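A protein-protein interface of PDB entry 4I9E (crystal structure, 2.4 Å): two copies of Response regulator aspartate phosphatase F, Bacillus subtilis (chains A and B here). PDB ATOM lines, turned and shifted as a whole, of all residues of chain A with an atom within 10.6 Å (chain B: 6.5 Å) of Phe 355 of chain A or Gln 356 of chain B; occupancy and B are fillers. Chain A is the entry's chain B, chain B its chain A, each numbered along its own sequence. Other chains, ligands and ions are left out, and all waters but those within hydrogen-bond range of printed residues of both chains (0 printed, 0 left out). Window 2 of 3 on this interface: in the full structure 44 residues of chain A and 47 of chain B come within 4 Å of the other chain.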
ATOM      1  N   VAL A 345     -19.167   3.614  -5.891  1.00  0.00           N
ATOM      2  CA  VAL A 345     -18.053   4.508  -5.986  1.00  0.00           C
ATOM      3  C   VAL A 345     -17.427   4.775  -4.622  1.00  0.00           C
ATOM      4  O   VAL A 345     -16.203   4.771  -4.499  1.00  0.00           O
ATOM      5  CB  VAL A 345     -18.408   5.873  -6.649  1.00  0.00           C
ATOM      6  CG1 VAL A 345     -17.108   6.732  -6.753  1.00  0.00           C
ATOM      7  CG2 VAL A 345     -18.968   5.702  -8.040  1.00  0.00           C
ATOM      8  N   ALA A 346     -18.252   5.041  -3.608  1.00  0.00           N
ATOM      9  CA  ALA A 346     -17.768   5.236  -2.233  1.00  0.00           C
ATOM     10  C   ALA A 346     -16.941   4.026  -1.738  1.00  0.00           C
ATOM     11  O   ALA A 346     -15.893   4.172  -1.103  1.00  0.00           O
ATOM     12  CB  ALA A 346     -18.920   5.478  -1.325  1.00  0.00           C
ATOM     13  N   LYS A 347     -17.415   2.828  -2.044  1.00  0.00           N
ATOM     14  CA  LYS A 347     -16.811   1.613  -1.509  1.00  0.00           C
ATOM     15  C   LYS A 347     -15.525   1.270  -2.244  1.00  0.00           C
ATOM     16  O   LYS A 347     -14.568   0.755  -1.661  1.00  0.00           O
ATOM     17  CB  LYS A 347     -17.806   0.465  -1.570  1.00  0.00           C
ATOM     18  CG  LYS A 347     -18.803   0.443  -0.416  1.00  0.00           C
ATOM     19  CD  LYS A 347     -19.963  -0.425  -0.848  1.00  0.00           C
ATOM     20  CE  LYS A 347     -20.324  -1.493   0.137  1.00  0.00           C
ATOM     21  NZ  LYS A 347     -21.281  -0.974   1.098  1.00  0.00           N
ATOM     22  N   TYR A 348     -15.482   1.591  -3.523  1.00  0.00           N
ATOM     23  CA  TYR A 348     -14.337   1.335  -4.302  1.00  0.00           C
ATOM     24  C   TYR A 348     -13.158   2.193  -3.813  1.00  0.00           C
ATOM     25  O   TYR A 348     -12.043   1.702  -3.695  1.00  0.00           O
ATOM     26  CB  TYR A 348     -14.674   1.609  -5.746  1.00  0.00           C
ATOM     27  CG  TYR A 348     -13.480   1.681  -6.676  1.00  0.00           C
ATOM     28  CD1 TYR A 348     -13.149   0.608  -7.476  1.00  0.00           C
ATOM     29  CD2 TYR A 348     -12.704   2.824  -6.763  1.00  0.00           C
ATOM     30  CE1 TYR A 348     -12.070   0.659  -8.333  1.00  0.00           C
ATOM     31  CE2 TYR A 348     -11.590   2.869  -7.608  1.00  0.00           C
ATOM     32  CZ  TYR A 348     -11.299   1.791  -8.394  1.00  0.00           C
ATOM     33  OH  TYR A 348     -10.235   1.827  -9.276  1.00  0.00           O
ATOM     34  N   TYR A 349     -13.420   3.480  -3.576  1.00  0.00           N
ATOM     35  CA  TYR A 349     -12.424   4.400  -3.010  1.00  0.00           C
ATOM     36  C   TYR A 349     -12.061   4.051  -1.574  1.00  0.00           C
ATOM     37  O   TYR A 349     -10.938   4.333  -1.162  1.00  0.00           O
ATOM     38  CB  TYR A 349     -12.907   5.858  -3.043  1.00  0.00           C
ATOM     39  CG  TYR A 349     -12.773   6.556  -4.391  1.00  0.00           C
ATOM     40  CD1 TYR A 349     -11.534   6.634  -5.072  1.00  0.00           C
ATOM     41  CD2 TYR A 349     -13.880   7.184  -4.960  1.00  0.00           C
ATOM     42  CE1 TYR A 349     -11.424   7.315  -6.285  1.00  0.00           C
ATOM     43  CE2 TYR A 349     -13.792   7.847  -6.157  1.00  0.00           C
ATOM     44  CZ  TYR A 349     -12.594   7.920  -6.825  1.00  0.00           C
ATOM     45  OH  TYR A 349     -12.605   8.599  -8.020  1.00  0.00           O
ATOM     46  N   HIS A 350     -13.025   3.483  -0.832  1.00  0.00           N
ATOM     47  CA  HIS A 350     -12.827   3.116   0.567  1.00  0.00           C
ATOM     48  C   HIS A 350     -11.869   1.936   0.670  1.00  0.00           C
ATOM     49  O   HIS A 350     -11.011   1.883   1.543  1.00  0.00           O
ATOM     50  CB  HIS A 350     -14.139   2.783   1.298  1.00  0.00           C
ATOM     51  CG  HIS A 350     -13.938   2.490   2.750  1.00  0.00           C
ATOM     52  ND1 HIS A 350     -13.849   3.487   3.704  1.00  0.00           N
ATOM     53  CD2 HIS A 350     -13.704   1.321   3.400  1.00  0.00           C
ATOM     54  CE1 HIS A 350     -13.614   2.940   4.886  1.00  0.00           C
ATOM     55  NE2 HIS A 350     -13.524   1.627   4.727  1.00  0.00           N
ATOM     56  N   GLU A 351     -12.036   0.990  -0.233  1.00  0.00           N
ATOM     57  CA  GLU A 351     -11.225  -0.183  -0.188  1.00  0.00           C
ATOM     58  C   GLU A 351      -9.792   0.162  -0.550  1.00  0.00           C
ATOM     59  O   GLU A 351      -8.867  -0.563  -0.186  1.00  0.00           O
ATOM     60  CB  GLU A 351     -11.733  -1.217  -1.136  1.00  0.00           C
ATOM     61  CG  GLU A 351     -11.160  -2.528  -0.775  1.00  0.00           C
ATOM     62  CD  GLU A 351     -11.521  -3.583  -1.764  1.00  0.00           C
ATOM     63  OE1 GLU A 351     -11.378  -3.319  -2.994  1.00  0.00           O
ATOM     64  OE2 GLU A 351     -11.950  -4.672  -1.296  1.00  0.00           O
ATOM     65  N   ARG A 352      -9.621   1.275  -1.253  1.00  0.00           N
ATOM     66  CA  ARG A 352      -8.323   1.732  -1.716  1.00  0.00           C
ATOM     67  C   ARG A 352      -7.754   2.781  -0.762  1.00  0.00           C
ATOM     68  O   ARG A 352      -6.758   3.433  -1.064  1.00  0.00           O
ATOM     69  CB  ARG A 352      -8.433   2.228  -3.171  1.00  0.00           C
ATOM     70  CG  ARG A 352      -8.569   1.052  -4.123  1.00  0.00           C
ATOM     71  CD  ARG A 352      -9.211   1.375  -5.454  1.00  0.00           C
ATOM     72  NE  ARG A 352      -9.291   0.136  -6.242  1.00  0.00           N
ATOM     73  CZ  ARG A 352      -8.392  -0.203  -7.172  1.00  0.00           C
ATOM     74  NH1 ARG A 352      -7.382   0.619  -7.447  1.00  0.00           N
ATOM     75  NH2 ARG A 352      -8.492  -1.345  -7.848  1.00  0.00           N
ATOM     76  N   LYS A 353      -8.398   2.900   0.398  1.00  0.00           N
ATOM     77  CA  LYS A 353      -8.026   3.810   1.478  1.00  0.00           C
ATOM     78  C   LYS A 353      -7.975   5.286   1.034  1.00  0.00           C
ATOM     79  O   LYS A 353      -7.296   6.138   1.681  1.00  0.00           O
ATOM     80  CB  LYS A 353      -6.713   3.380   2.175  1.00  0.00           C
ATOM     81  CG  LYS A 353      -6.716   1.982   2.759  1.00  0.00           C
ATOM     82  CD  LYS A 353      -5.758   1.130   1.958  1.00  0.00           C
ATOM     83  CE  LYS A 353      -6.131  -0.356   1.983  1.00  0.00           C
ATOM     84  NZ  LYS A 353      -6.847  -0.764   3.235  1.00  0.00           N
ATOM     85  N   ASN A 354      -8.684   5.598  -0.056  1.00  0.00           N
ATOM     86  CA  ASN A 354      -8.932   6.992  -0.364  1.00  0.00           C
ATOM     87  C   ASN A 354     -10.206   7.365   0.358  1.00  0.00           C
ATOM     88  O   ASN A 354     -11.271   7.314  -0.207  1.00  0.00           O
ATOM     89  CB  ASN A 354      -8.977   7.260  -1.870  1.00  0.00           C
ATOM     90  CG  ASN A 354      -8.823   8.745  -2.224  1.00  0.00           C
ATOM     91  OD1 ASN A 354      -9.013   9.654  -1.379  1.00  0.00           O
ATOM     92  ND2 ASN A 354      -8.520   9.004  -3.511  1.00  0.00           N
ATOM     93  N   PHE A 355     -10.060   7.723   1.634  1.00  0.00           N
ATOM     94  CA  PHE A 355     -11.171   8.025   2.516  1.00  0.00           C
ATOM     95  C   PHE A 355     -11.785   9.408   2.245  1.00  0.00           C
ATOM     96  O   PHE A 355     -12.935   9.647   2.583  1.00  0.00           O
ATOM     97  CB  PHE A 355     -10.751   7.919   3.999  1.00  0.00           C
ATOM     98  CG  PHE A 355     -10.065   6.633   4.366  1.00  0.00           C
ATOM     99  CD1 PHE A 355     -10.781   5.441   4.470  1.00  0.00           C
ATOM    100  CD2 PHE A 355      -8.682   6.615   4.616  1.00  0.00           C
ATOM    101  CE1 PHE A 355     -10.128   4.234   4.825  1.00  0.00           C
ATOM    102  CE2 PHE A 355      -8.025   5.416   4.969  1.00  0.00           C
ATOM    103  CZ  PHE A 355      -8.751   4.235   5.074  1.00  0.00           C
ATOM    104  N   GLN A 356     -11.024  10.329   1.677  1.00  0.00           N
ATOM    105  CA  GLN A 356     -11.596  11.637   1.358  1.00  0.00           C
ATOM    106  C   GLN A 356     -12.633  11.559   0.269  1.00  0.00           C
ATOM    107  O   GLN A 356     -13.626  12.286   0.291  1.00  0.00           O
ATOM    108  CB  GLN A 356     -10.540  12.563   0.834  1.00  0.00           C
ATOM    109  CG  GLN A 356     -10.987  14.000   0.714  1.00  0.00           C
ATOM    110  CD  GLN A 356      -9.775  14.932   0.677  1.00  0.00           C
ATOM    111  OE1 GLN A 356      -8.602  14.476   0.814  1.00  0.00           O
ATOM    112  NE2 GLN A 356     -10.036  16.236   0.503  1.00  0.00           N
ATOM    113  N   LYS A 357     -12.318  10.727  -0.722  1.00  0.00           N
ATOM    114  CA  LYS A 357     -13.127  10.576  -1.915  1.00  0.00           C
ATOM    115  C   LYS A 357     -14.315   9.647  -1.676  1.00  0.00           C
ATOM    116  O   LYS A 357     -15.415   9.923  -2.118  1.00  0.00           O
ATOM    117  CB  LYS A 357     -12.245  10.116  -3.071  1.00  0.00           C
ATOM    118  CG  LYS A 357     -11.644  11.322  -3.767  1.00  0.00           C
ATOM    119  CD  LYS A 357     -10.958  10.953  -5.044  1.00  0.00           C
ATOM    120  CE  LYS A 357     -10.192  12.160  -5.612  1.00  0.00           C
ATOM    121  NZ  LYS A 357     -11.086  13.357  -5.600  1.00  0.00           N
ATOM    122  N   ALA A 358     -14.072   8.561  -0.958  1.00  0.00           N
ATOM    123  CA  ALA A 358     -15.122   7.706  -0.397  1.00  0.00           C
ATOM    124  C   ALA A 358     -16.144   8.537   0.334  1.00  0.00           C
ATOM    125  O   ALA A 358     -17.323   8.363   0.188  1.00  0.00           O
ATOM    126  CB  ALA A 358     -14.502   6.675   0.522  1.00  0.00           C
ATOM    127  N   SER A 359     -15.669   9.457   1.136  1.00  0.00           N
ATOM    128  CA  SER A 359     -16.482  10.243   2.000  1.00  0.00           C
ATOM    129  C   SER A 359     -17.266  11.260   1.196  1.00  0.00           C
ATOM    130  O   SER A 359     -18.347  11.706   1.591  1.00  0.00           O
ATOM    131  CB  SER A 359     -15.559  10.929   2.998  1.00  0.00           C
ATOM    132  OG  SER A 359     -16.284  11.618   3.987  1.00  0.00           O
ATOM    133  N   ALA A 360     -16.743  11.617   0.035  1.00  0.00           N
ATOM    134  CA  ALA A 360     -17.438  12.565  -0.800  1.00  0.00           C
ATOM    135  C   ALA A 360     -18.605  11.873  -1.506  1.00  0.00           C
ATOM    136  O   ALA A 360     -19.663  12.453  -1.633  1.00  0.00           O
ATOM    137  CB  ALA A 360     -16.493  13.187  -1.780  1.00  0.00           C
ATOM    138  N   TYR A 361     -18.415  10.650  -1.976  1.00  0.00           N
ATOM    139  CA  TYR A 361     -19.493   9.868  -2.573  1.00  0.00           C
ATOM    140  C   TYR A 361     -20.490   9.337  -1.532  1.00  0.00           C
ATOM    141  O   TYR A 361     -21.648   9.171  -1.851  1.00  0.00           O
ATOM    142  CB  TYR A 361     -18.927   8.740  -3.421  1.00  0.00           C
ATOM    143  CG  TYR A 361     -18.343   9.282  -4.684  1.00  0.00           C
ATOM    144  CD1 TYR A 361     -19.178   9.597  -5.784  1.00  0.00           C
ATOM    145  CD2 TYR A 361     -16.972   9.549  -4.785  1.00  0.00           C
ATOM    146  CE1 TYR A 361     -18.667  10.117  -6.919  1.00  0.00           C
ATOM    147  CE2 TYR A 361     -16.435  10.102  -5.958  1.00  0.00           C
ATOM    148  CZ  TYR A 361     -17.290  10.377  -7.007  1.00  0.00           C
ATOM    149  OH  TYR A 361     -16.792  10.926  -8.156  1.00  0.00           O
ATOM    150  N   PHE A 362     -20.054   9.076  -0.292  1.00  0.00           N
ATOM    151  CA  PHE A 362     -21.010   8.817   0.771  1.00  0.00           C
ATOM    152  C   PHE A 362     -21.923  10.040   0.946  1.00  0.00           C
ATOM    153  O   PHE A 362     -23.095   9.896   1.261  1.00  0.00           O
ATOM    154  CB  PHE A 362     -20.349   8.441   2.081  1.00  0.00           C
ATOM    155  CG  PHE A 362     -19.809   7.027   2.121  1.00  0.00           C
ATOM    156  CD1 PHE A 362     -20.635   5.927   1.852  1.00  0.00           C
ATOM    157  CD2 PHE A 362     -18.480   6.794   2.473  1.00  0.00           C
ATOM    158  CE1 PHE A 362     -20.145   4.633   1.903  1.00  0.00           C
ATOM    159  CE2 PHE A 362     -17.972   5.502   2.522  1.00  0.00           C
ATOM    160  CZ  PHE A 362     -18.789   4.420   2.235  1.00  0.00           C
ATOM    161  N   LEU A 363     -21.397  11.246   0.724  1.00  0.00           N
ATOM    162  CA  LEU A 363     -22.245  12.450   0.810  1.00  0.00           C
ATOM    163  C   LEU A 363     -23.154  12.667  -0.400  1.00  0.00           C
ATOM    164  O   LEU A 363     -24.218  13.206  -0.262  1.00  0.00           O
ATOM    165  CB  LEU A 363     -21.406  13.684   1.090  1.00  0.00           C
ATOM    166  CG  LEU A 363     -20.934  13.764   2.547  1.00  0.00           C
ATOM    167  CD1 LEU A 363     -19.635  14.602   2.564  1.00  0.00           C
ATOM    168  CD2 LEU A 363     -22.026  14.364   3.413  1.00  0.00           C
ATOM    169  N   HIS B 350     -16.335  14.284   9.072  1.00  0.00           N
ATOM    170  CA  HIS B 350     -16.104  14.782   7.733  1.00  0.00           C
ATOM    171  C   HIS B 350     -15.659  16.217   7.774  1.00  0.00           C
ATOM    172  O   HIS B 350     -14.674  16.563   7.116  1.00  0.00           O
ATOM    173  CB  HIS B 350     -17.324  14.677   6.822  1.00  0.00           C
ATOM    174  CG  HIS B 350     -17.043  15.135   5.426  1.00  0.00           C
ATOM    175  ND1 HIS B 350     -16.517  14.300   4.465  1.00  0.00           N
ATOM    176  CD2 HIS B 350     -17.129  16.355   4.853  1.00  0.00           C
ATOM    177  CE1 HIS B 350     -16.318  14.975   3.348  1.00  0.00           C
ATOM    178  NE2 HIS B 350     -16.680  16.227   3.556  1.00  0.00           N
ATOM    179  N   LYS B 353     -12.079  16.688   8.601  1.00  0.00           N
ATOM    180  CA  LYS B 353     -11.126  16.055   7.697  1.00  0.00           C
ATOM    181  C   LYS B 353     -10.673  14.689   8.172  1.00  0.00           C
ATOM    182  O   LYS B 353      -9.743  14.089   7.606  1.00  0.00           O
ATOM    183  CB  LYS B 353      -9.921  16.963   7.421  1.00  0.00           C
ATOM    184  CG  LYS B 353     -10.184  18.142   6.465  1.00  0.00           C
ATOM    185  CD  LYS B 353     -11.030  19.250   7.112  1.00  0.00           C
ATOM    186  CE  LYS B 353     -11.023  20.513   6.256  1.00  0.00           C
ATOM    187  NZ  LYS B 353     -11.940  20.329   5.119  1.00  0.00           N
ATOM    188  N   ASN B 354     -11.293  14.187   9.227  1.00  0.00           N
ATOM    189  CA  ASN B 354     -11.081  12.808   9.557  1.00  0.00           C
ATOM    190  C   ASN B 354     -11.950  11.920   8.620  1.00  0.00           C
ATOM    191  O   ASN B 354     -13.004  11.363   9.006  1.00  0.00           O
ATOM    192  CB  ASN B 354     -11.367  12.576  11.012  1.00  0.00           C
ATOM    193  CG  ASN B 354     -10.778  11.296  11.493  1.00  0.00           C
ATOM    194  OD1 ASN B 354     -10.537  10.360  10.717  1.00  0.00           O
ATOM    195  ND2 ASN B 354     -10.528  11.228  12.787  1.00  0.00           N
ATOM    196  N   PHE B 355     -11.487  11.805   7.376  1.00  0.00           N
ATOM    197  CA  PHE B 355     -12.206  11.134   6.335  1.00  0.00           C
ATOM    198  C   PHE B 355     -12.303   9.630   6.576  1.00  0.00           C
ATOM    199  O   PHE B 355     -13.278   8.981   6.123  1.00  0.00           O
ATOM    200  CB  PHE B 355     -11.577  11.452   4.978  1.00  0.00           C
ATOM    201  CG  PHE B 355     -11.555  12.923   4.655  1.00  0.00           C
ATOM    202  CD1 PHE B 355     -12.756  13.631   4.483  1.00  0.00           C
ATOM    203  CD2 PHE B 355     -10.335  13.610   4.541  1.00  0.00           C
ATOM    204  CE1 PHE B 355     -12.755  14.999   4.216  1.00  0.00           C
ATOM    205  CE2 PHE B 355     -10.321  14.984   4.257  1.00  0.00           C
ATOM    206  CZ  PHE B 355     -11.536  15.687   4.076  1.00  0.00           C
ATOM    207  N   GLN B 356     -11.318   9.082   7.289  1.00  0.00           N
ATOM    208  CA  GLN B 356     -11.343   7.662   7.576  1.00  0.00           C
ATOM    209  C   GLN B 356     -12.423   7.337   8.592  1.00  0.00           C
ATOM    210  O   GLN B 356     -13.060   6.292   8.477  1.00  0.00           O
ATOM    211  CB  GLN B 356      -9.977   7.146   8.017  1.00  0.00           C
ATOM    212  CG  GLN B 356      -9.918   5.623   8.298  1.00  0.00           C
ATOM    213  CD  GLN B 356      -8.484   5.111   8.629  1.00  0.00           C
ATOM    214  OE1 GLN B 356      -7.466   5.840   8.493  1.00  0.00           O
ATOM    215  NE2 GLN B 356      -8.407   3.831   9.044  1.00  0.00           N
ATOM    216  N   LYS B 357     -12.634   8.238   9.560  1.00  0.00           N
ATOM    217  CA  LYS B 357     -13.714   8.100  10.554  1.00  0.00           C
ATOM    218  C   LYS B 357     -15.100   8.412   9.958  1.00  0.00           C
ATOM    219  O   LYS B 357     -16.060   7.680  10.229  1.00  0.00           O
ATOM    220  CB  LYS B 357     -13.493   9.004  11.803  1.00  0.00           C
ATOM    221  CG  LYS B 357     -12.380   8.593  12.841  1.00  0.00           C
ATOM    222  CD  LYS B 357     -12.497   7.170  13.341  1.00  0.00           C
ATOM    223  CE  LYS B 357     -11.381   6.883  14.337  1.00  0.00           C
ATOM    224  NZ  LYS B 357     -11.449   5.449  14.813  1.00  0.00           N
ATOM    225  N   ALA B 358     -15.201   9.522   9.221  1.00  0.00           N
ATOM    226  CA  ALA B 358     -16.433   9.941   8.554  1.00  0.00           C
ATOM    227  C   ALA B 358     -16.965   8.734   7.775  1.00  0.00           C
ATOM    228  O   ALA B 358     -18.085   8.315   7.918  1.00  0.00           O
ATOM    229  CB  ALA B 358     -16.163  11.125   7.625  1.00  0.00           C
ATOM    230  N   SER B 359     -16.065   8.119   7.044  1.00  0.00           N
ATOM    231  CA  SER B 359     -16.327   7.044   6.168  1.00  0.00           C
ATOM    232  C   SER B 359     -16.784   5.777   6.892  1.00  0.00           C
ATOM    233  O   SER B 359     -17.758   5.140   6.448  1.00  0.00           O
ATOM    234  CB  SER B 359     -15.098   6.913   5.292  1.00  0.00           C
ATOM    235  OG  SER B 359     -14.970   5.682   4.675  1.00  0.00           O
ATOM    236  N   ALA B 360     -16.175   5.436   8.036  1.00  0.00           N
ATOM    237  CA  ALA B 360     -16.591   4.267   8.863  1.00  0.00           C
ATOM    238  C   ALA B 360     -18.030   4.392   9.373  1.00  0.00           C
ATOM    239  O   ALA B 360     -18.770   3.428   9.392  1.00  0.00           O
ATOM    240  CB  ALA B 360     -15.600   4.017  10.081  1.00  0.00           C
ATOM    241  N   TYR B 361     -18.405   5.597   9.783  1.00  0.00           N
ATOM    242  CA  TYR B 361     -19.761   5.910  10.171  1.00  0.00           C
ATOM    243  C   TYR B 361     -20.763   5.983   8.986  1.00  0.00           C
ATOM    244  O   TYR B 361     -21.933   5.688   9.169  1.00  0.00           O
ATOM    245  CB  TYR B 361     -19.771   7.202  11.011  1.00  0.00           C
ATOM    246  CG  TYR B 361     -19.244   6.943  12.374  1.00  0.00           C
ATOM    247  CD1 TYR B 361     -20.019   6.274  13.304  1.00  0.00           C
ATOM    248  CD2 TYR B 361     -17.930   7.284  12.721  1.00  0.00           C
ATOM    249  CE1 TYR B 361     -19.533   5.988  14.584  1.00  0.00           C
ATOM    250  CE2 TYR B 361     -17.412   7.000  14.015  1.00  0.00           C
ATOM    251  CZ  TYR B 361     -18.229   6.359  14.940  1.00  0.00           C
ATOM    252  OH  TYR B 361     -17.780   6.035  16.210  1.00  0.00           O
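Phe 355 of chain A touches Phe 355 of chain B.
Phe 355 of chain A touches Gln 356 of chain B.
Gln 356 of chain A touches Phe 355 of chain B.
OG of Ser 359 of chain A touches CB of Ala 358 of chain B (3.7 Å).
CE2 of Phe 362 of chain A touches OG of Ser 359 of chain B, at 3.7 Å.
His 350 of chain B touches Leu 363 of chain A.
Printed residues of chain B that touch a printed residue of chain A: His 350, Phe 355, Gln 356, Ala 358 and Ser 359.
Among the printed residues, 8 pairs touch across the chains.
Among the printed residues, no Asp or Glu carboxylate lies within 4 Å of a Lys or Arg side-chain nitrogen of the other chain.
The side-chain hydroxyl (OG) of Ser 359 of chain A is in hydrogen-bond range of a ring nitrogen (ND1) of His 350 of chain B (2.7 Å).
ND1 of His 350 of chain A lies within hydrogen-bond range of OG of Ser 359 of chain B (2.6 Å).
Phe 355 of chain A touches just these residues of chain B: Phe 355 (3.3 Å) and Gln 356 (3.5 Å).
No residue of chain A comes within 4 Å of Asn 354 of chain B.
Phe 355 of chain B touches just these residues of chain A: Phe 355 and Gln 356.
Of chain A, only Ser 359 (3.7 Å) comes within 4 Å of Ala 358 of chain B.
Of the printed residues of chain A, Ser 359 of chain B touches His 350 and Phe 362.
No residue of chain A comes within 4 Å of Ala 360 of chain B.
Of the printed residues of chain B, Phe 362 of chain A touches Ser 359 (3.7 Å).
Of the printed residues of chain B, His 350 of chain A touches Ser 359.
Of the printed residues of chain B, Leu 363 of chain A touches His 350 (3.4 Å).
Of the printed residues of chain B, Ser 359 of chain A touches His 350 (2.7 Å) and Ala 358 (3.7 Å).
Of the printed residues of chain B, Gln 356 of chain A touches Phe 355.
The nearest residue of chain B that does not touch Phe 355 of chain A is Ser 359 of chain B (4.2 Å).
The nearest residue of chain A that does not touch Gln 356 of chain B is His 350 of chain A (4.9 Å).
The nearest printed residue of chain B that does not touch Phe 362 of chain A is Ala 358 of chain B (5.7 Å).
His 350 of chain A touches Ser 359 of chain B, and with the chains exchanged Ser 359 of chain A touches His 350 of chain B.
Phe 355 of chain A touches its own counterpart, Phe 355 of chain B.
Phe 355 of chain A touches Gln 356 of chain B, and with the chains exchanged Gln 356 of chain A touches Phe 355 of chain B.
Ser 359 of chain A touches Ala 358 of chain B, but with the chains exchanged Ala 358 of chain A does not touch Ser 359 of chain B (4.3 Å).
10 positions are printed for both chains.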
